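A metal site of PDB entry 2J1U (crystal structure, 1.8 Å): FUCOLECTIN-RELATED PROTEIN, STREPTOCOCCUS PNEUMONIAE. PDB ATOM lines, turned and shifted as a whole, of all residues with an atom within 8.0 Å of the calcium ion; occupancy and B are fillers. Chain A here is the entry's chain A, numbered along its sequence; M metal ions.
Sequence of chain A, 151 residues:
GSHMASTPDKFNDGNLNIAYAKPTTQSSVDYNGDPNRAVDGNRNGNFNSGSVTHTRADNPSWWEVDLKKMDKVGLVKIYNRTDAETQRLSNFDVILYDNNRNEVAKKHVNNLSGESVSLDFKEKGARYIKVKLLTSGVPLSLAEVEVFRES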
ATOM      1  N   ASP A  34      -6.678   5.954  18.937  1.00  0.00           N
ATOM      2  CA  ASP A  34      -7.998   5.581  18.404  1.00  0.00           C
ATOM      3  C   ASP A  34      -8.319   6.258  17.047  1.00  0.00           C
ATOM      4  O   ASP A  34      -7.808   7.337  16.766  1.00  0.00           O
ATOM      5  CB  ASP A  34      -9.100   5.938  19.388  1.00  0.00           C
ATOM      6  CG  ASP A  34      -9.018   5.167  20.685  1.00  0.00           C
ATOM      7  OD1 ASP A  34      -8.842   3.932  20.629  1.00  0.00           O
ATOM      8  OD2 ASP A  34      -9.151   5.722  21.793  1.00  0.00           O
ATOM      9  N   PRO A  35      -9.101   5.598  16.211  1.00  0.00           N
ATOM     10  CA  PRO A  35      -9.332   6.036  14.834  1.00  0.00           C
ATOM     11  C   PRO A  35     -10.002   7.380  14.726  1.00  0.00           C
ATOM     12  O   PRO A  35      -9.780   8.110  13.737  1.00  0.00           O
ATOM     13  CB  PRO A  35     -10.194   4.915  14.242  1.00  0.00           C
ATOM     14  CG  PRO A  35     -10.684   4.215  15.337  1.00  0.00           C
ATOM     15  CD  PRO A  35      -9.709   4.296  16.475  1.00  0.00           C
ATOM     16  N   ASN A  36     -10.754   7.751  15.756  1.00  0.00           N
ATOM     17  CA  ASN A  36     -11.443   9.021  15.739  1.00  0.00           C
ATOM     18  C   ASN A  36     -10.516  10.257  15.833  1.00  0.00           C
ATOM     19  O   ASN A  36     -10.938  11.381  15.538  1.00  0.00           O
ATOM     20  CB  ASN A  36     -12.618   9.014  16.744  1.00  0.00           C
ATOM     21  CG  ASN A  36     -12.177   9.162  18.212  1.00  0.00           C
ATOM     22  OD1 ASN A  36     -12.991   9.556  19.076  1.00  0.00           O
ATOM     23  ND2 ASN A  36     -10.954   8.777  18.514  1.00  0.00           N
ATOM     24  N   ARG A  37      -9.269  10.014  16.173  1.00  0.00           N
ATOM     25  CA  ARG A  37      -8.287  11.085  16.185  1.00  0.00           C
ATOM     26  C   ARG A  37      -7.996  11.652  14.813  1.00  0.00           C
ATOM     27  O   ARG A  37      -7.557  12.779  14.746  1.00  0.00           O
ATOM     28  CB  ARG A  37      -7.005  10.614  16.899  1.00  0.00           C
ATOM     29  CG  ARG A  37      -7.252  10.435  18.369  1.00  0.00           C
ATOM     30  CD  ARG A  37      -6.025  10.000  19.150  1.00  0.00           C
ATOM     31  NE  ARG A  37      -6.432   9.566  20.499  1.00  0.00           N
ATOM     32  CZ  ARG A  37      -5.636   9.432  21.541  1.00  0.00           C
ATOM     33  NH1 ARG A  37      -6.159   9.058  22.725  1.00  0.00           N
ATOM     34  NH2 ARG A  37      -4.341   9.652  21.412  1.00  0.00           N
ATOM     35  N   ALA A  38      -8.290  10.923  13.724  1.00  0.00           N
ATOM     36  CA  ALA A  38      -8.112  11.452  12.372  1.00  0.00           C
ATOM     37  C   ALA A  38      -9.313  12.213  11.843  1.00  0.00           C
ATOM     38  O   ALA A  38      -9.287  12.651  10.685  1.00  0.00           O
ATOM     39  CB  ALA A  38      -7.767  10.348  11.365  1.00  0.00           C
ATOM     40  N   VAL A  39     -10.370  12.322  12.619  1.00  0.00           N
ATOM     41  CA  VAL A  39     -11.520  13.146  12.221  1.00  0.00           C
ATOM     42  C   VAL A  39     -11.935  14.098  13.344  1.00  0.00           C
ATOM     43  O   VAL A  39     -13.126  14.488  13.451  1.00  0.00           O
ATOM     44  CB  VAL A  39     -12.765  12.287  11.720  1.00  0.00           C
ATOM     45  CG1 VAL A  39     -12.462  11.468  10.466  1.00  0.00           C
ATOM     46  CG2 VAL A  39     -13.312  11.346  12.803  1.00  0.00           C
ATOM     47  N   ASP A  40     -10.979  14.494  14.187  1.00  0.00           N
ATOM     48  CA  ASP A  40     -11.333  15.387  15.288  1.00  0.00           C
ATOM     49  C   ASP A  40     -11.161  16.875  14.964  1.00  0.00           C
ATOM     50  O   ASP A  40     -11.274  17.708  15.878  1.00  0.00           O
ATOM     51  CB  ASP A  40     -10.603  15.041  16.562  1.00  0.00           C
ATOM     52  CG  ASP A  40      -9.076  15.161  16.448  1.00  0.00           C
ATOM     53  OD1 ASP A  40      -8.504  15.548  15.403  1.00  0.00           O
ATOM     54  OD2 ASP A  40      -8.377  14.843  17.403  1.00  0.00           O
ATOM     55  N   GLY A  41     -10.856  17.186  13.712  1.00  0.00           N
ATOM     56  CA  GLY A  41     -10.712  18.584  13.270  1.00  0.00           C
ATOM     57  C   GLY A  41      -9.359  19.187  13.574  1.00  0.00           C
ATOM     58  O   GLY A  41      -9.141  20.358  13.259  1.00  0.00           O
ATOM     59  N   ASN A  42      -8.451  18.392  14.153  1.00  0.00           N
ATOM     60  CA  ASN A  42      -7.118  18.804  14.596  1.00  0.00           C
ATOM     61  C   ASN A  42      -6.018  18.184  13.718  1.00  0.00           C
ATOM     62  O   ASN A  42      -5.813  16.938  13.689  1.00  0.00           O
ATOM     63  CB  ASN A  42      -6.939  18.436  16.063  1.00  0.00           C
ATOM     64  CG  ASN A  42      -5.612  18.944  16.645  1.00  0.00           C
ATOM     65  OD1 ASN A  42      -4.833  19.582  15.957  1.00  0.00           O
ATOM     66  ND2 ASN A  42      -5.441  18.748  17.915  1.00  0.00           N
ATOM     67  N   ARG A  43      -5.333  19.033  12.974  1.00  0.00           N
ATOM     68  CA  ARG A  43      -4.280  18.513  12.045  1.00  0.00           C
ATOM     69  C   ARG A  43      -2.870  18.308  12.659  1.00  0.00           C
ATOM     70  O   ARG A  43      -1.925  17.927  11.935  1.00  0.00           O
ATOM     71  CB  ARG A  43      -4.136  19.426  10.844  1.00  0.00           C
ATOM     72  CG  ARG A  43      -5.423  19.625  10.038  1.00  0.00           C
ATOM     73  CD  ARG A  43      -5.244  20.874   9.114  1.00  0.00           C
ATOM     74  NE  ARG A  43      -6.307  21.028   8.133  1.00  0.00           N
ATOM     75  CZ  ARG A  43      -6.264  21.979   7.174  1.00  0.00           C
ATOM     76  NH1 ARG A  43      -7.249  22.053   6.278  1.00  0.00           N
ATOM     77  NH2 ARG A  43      -5.240  22.832   7.092  1.00  0.00           N
ATOM     78  N   ASN A  44      -2.741  18.603  13.963  1.00  0.00           N
ATOM     79  CA  ASN A  44      -1.469  18.534  14.690  1.00  0.00           C
ATOM     80  C   ASN A  44      -0.975  17.091  14.531  1.00  0.00           C
ATOM     81  O   ASN A  44      -1.693  16.129  14.879  1.00  0.00           O
ATOM     82  CB  ASN A  44      -1.663  18.926  16.175  1.00  0.00           C
ATOM     83  CG  ASN A  44      -0.368  19.010  16.987  1.00  0.00           C
ATOM     84  OD1 ASN A  44      -0.331  19.583  18.129  1.00  0.00           O
ATOM     85  ND2 ASN A  44       0.678  18.468  16.464  1.00  0.00           N
ATOM     86  N   GLY A  45       0.175  16.940  13.903  1.00  0.00           N
ATOM     87  CA  GLY A  45       0.735  15.615  13.645  1.00  0.00           C
ATOM     88  C   GLY A  45       1.678  15.084  14.702  1.00  0.00           C
ATOM     89  O   GLY A  45       2.320  14.055  14.469  1.00  0.00           O
ATOM     90  N   GLY A  50      -1.866  13.996  20.978  1.00  0.00           N
ATOM     91  CA  GLY A  50      -3.141  13.325  21.123  1.00  0.00           C
ATOM     92  C   GLY A  50      -4.104  13.294  19.958  1.00  0.00           C
ATOM     93  O   GLY A  50      -5.185  12.720  20.080  1.00  0.00           O
ATOM     94  N   SER A  51      -3.709  13.861  18.807  1.00  0.00           N
ATOM     95  CA  SER A  51      -4.575  14.050  17.641  1.00  0.00           C
ATOM     96  C   SER A  51      -4.186  13.121  16.488  1.00  0.00           C
ATOM     97  O   SER A  51      -4.655  13.330  15.391  1.00  0.00           O
ATOM     98  CB  SER A  51      -4.518  15.531  17.192  1.00  0.00           C
ATOM     99  OG  SER A  51      -4.062  15.701  15.861  1.00  0.00           O
ATOM    100  N   VAL A  52      -3.376  12.094  16.769  1.00  0.00           N
ATOM    101  CA  VAL A  52      -2.887  11.185  15.712  1.00  0.00           C
ATOM    102  C   VAL A  52      -3.284   9.726  16.049  1.00  0.00           C
ATOM    103  O   VAL A  52      -3.131   9.312  17.168  1.00  0.00           O
ATOM    104  CB  VAL A  52      -1.400  11.315  15.590  1.00  0.00           C
ATOM    105  CG1 VAL A  52      -0.821  10.452  14.472  1.00  0.00           C
ATOM    106  CG2 VAL A  52      -0.914  12.774  15.340  1.00  0.00           C
ATOM    107  N   THR A  53      -3.773   8.988  15.052  1.00  0.00           N
ATOM    108  CA  THR A  53      -4.127   7.606  15.236  1.00  0.00           C
ATOM    109  C   THR A  53      -2.854   6.732  15.291  1.00  0.00           C
ATOM    110  O   THR A  53      -1.768   7.154  14.898  1.00  0.00           O
ATOM    111  CB  THR A  53      -4.995   7.097  14.094  1.00  0.00           C
ATOM    112  OG1 THR A  53      -4.242   7.074  12.860  1.00  0.00           O
ATOM    113  CG2 THR A  53      -6.217   8.004  13.821  1.00  0.00           C
ATOM    114  N   TYR A  79      -3.272  14.095   6.291  1.00  0.00           N
ATOM    115  CA  TYR A  79      -2.208  14.682   7.083  1.00  0.00           C
ATOM    116  C   TYR A  79      -1.488  13.594   7.839  1.00  0.00           C
ATOM    117  O   TYR A  79      -2.099  12.836   8.583  1.00  0.00           O
ATOM    118  CB  TYR A  79      -2.749  15.772   8.000  1.00  0.00           C
ATOM    119  CG  TYR A  79      -3.319  16.994   7.268  1.00  0.00           C
ATOM    120  CD1 TYR A  79      -2.582  18.159   7.144  1.00  0.00           C
ATOM    121  CD2 TYR A  79      -4.611  16.970   6.687  1.00  0.00           C
ATOM    122  CE1 TYR A  79      -3.043  19.254   6.488  1.00  0.00           C
ATOM    123  CE2 TYR A  79      -5.086  18.100   6.004  1.00  0.00           C
ATOM    124  CZ  TYR A  79      -4.282  19.232   5.918  1.00  0.00           C
ATOM    125  OH  TYR A  79      -4.658  20.370   5.267  1.00  0.00           O
ATOM    126  N   LEU A 142      -2.262   8.465  11.340  1.00  0.00           N
ATOM    127  CA  LEU A 142      -2.766   9.533  10.529  1.00  0.00           C
ATOM    128  C   LEU A 142      -3.126  10.670  11.492  1.00  0.00           C
ATOM    129  O   LEU A 142      -3.786  10.473  12.542  1.00  0.00           O
ATOM    130  CB  LEU A 142      -4.017   9.082   9.775  1.00  0.00           C
ATOM    131  CG  LEU A 142      -3.886   7.929   8.780  1.00  0.00           C
ATOM    132  CD1 LEU A 142      -5.197   7.267   8.428  1.00  0.00           C
ATOM    133  CD2 LEU A 142      -3.166   8.441   7.478  1.00  0.00           C
ATOM    134  N   ALA A 143      -2.612  11.850  11.195  1.00  0.00           N
ATOM    135  CA  ALA A 143      -2.996  13.028  11.990  1.00  0.00           C
ATOM    136  C   ALA A 143      -4.421  13.504  11.742  1.00  0.00           C
ATOM    137  O   ALA A 143      -5.160  13.953  12.693  1.00  0.00           O
ATOM    138  CB  ALA A 143      -2.006  14.146  11.722  1.00  0.00           C
ATOM    139  N   GLU A 144      -4.817  13.435  10.478  1.00  0.00           N
ATOM    140  CA  GLU A 144      -6.146  13.852  10.068  1.00  0.00           C
ATOM    141  C   GLU A 144      -6.446  13.420   8.656  1.00  0.00           C
ATOM    142  O   GLU A 144      -5.564  13.473   7.765  1.00  0.00           O
ATOM    143  CB  GLU A 144      -6.331  15.375  10.204  1.00  0.00           C
ATOM    144  CG  GLU A 144      -7.796  15.850  10.162  1.00  0.00           C
ATOM    145  CD  GLU A 144      -8.573  15.608  11.458  1.00  0.00           C
ATOM    146  OE1 GLU A 144      -7.992  15.129  12.449  1.00  0.00           O
ATOM    147  OE2 GLU A 144      -9.796  15.914  11.476  1.00  0.00           O
ATOM    148  N   VAL A 145      -7.699  13.023   8.442  1.00  0.00           N
ATOM    149  CA  VAL A 145      -8.142  12.730   7.073  1.00  0.00           C
ATOM    150  C   VAL A 145      -9.360  13.591   6.801  1.00  0.00           C
ATOM    151  O   VAL A 145     -10.360  13.477   7.476  1.00  0.00           O
ATOM    152  CB  VAL A 145      -8.445  11.265   6.869  1.00  0.00           C
ATOM    153  CG1 VAL A 145      -8.974  10.995   5.454  1.00  0.00           C
ATOM    154  CG2 VAL A 145      -7.178  10.432   7.165  1.00  0.00           C
ATOM    155  N   GLU A 146      -9.200  14.488   5.847  1.00  0.00           N
ATOM    156  CA  GLU A 146     -10.254  15.425   5.477  1.00  0.00           C
ATOM    157  C   GLU A 146     -10.828  15.093   4.102  1.00  0.00           C
ATOM    158  O   GLU A 146     -10.128  14.783   3.157  1.00  0.00           O
ATOM    159  CB  GLU A 146      -9.722  16.858   5.503  1.00  0.00           C
ATOM    160  CG  GLU A 146      -9.201  17.286   6.876  1.00  0.00           C
ATOM    161  CD  GLU A 146      -8.586  18.662   6.923  1.00  0.00           C
ATOM    162  OE1 GLU A 146      -8.373  19.262   5.833  1.00  0.00           O
ATOM    163  OE2 GLU A 146      -8.248  19.102   8.053  1.00  0.00           O
HETATM  164 CA    CA M   1      -6.449  14.768  14.290  1.00  0.00          CA
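The backbone carbonyl oxygen of Tyr 79 lies within hydrogen-bond range of the backbone NH of Ala 143, 2.8 Å away. NE of Arg 37 sits close to O of Gly 50 (3.4 Å). The side-chain amide oxygen of Asn 42 sits at hydrogen-bond distance from the backbone NH of Asn 44, 3.1 Å away. The side-chain carboxylate of Glu 144 sits at hydrogen-bond distance from the backbone NH of Gly 41 (2.8 Å). The backbone NH (N) of Tyr 79 sits at hydrogen-bond distance from the backbone carbonyl oxygen (O) of Glu 144 (2.8 Å). OG of Ser 51 is in hydrogen-bond range of O of Asn 44 (2.6 Å).
The nearest printed residue that does not touch the calcium ion is Ala 38 (4.2 Å).
The calcium ion is bound by O of Ala 143 (2.2 Å), O of Arg 37 (2.3 Å), O of Asn 42 (2.3 Å), OE1 of Glu 144 (2.4 Å), OD1 of Asp 40 (2.5 Å) and O of Ser 51 (2.5 Å). Slightly farther from the calcium ion lies the side-chain hydroxyl (OG) of Ser 51 (3.0 Å).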
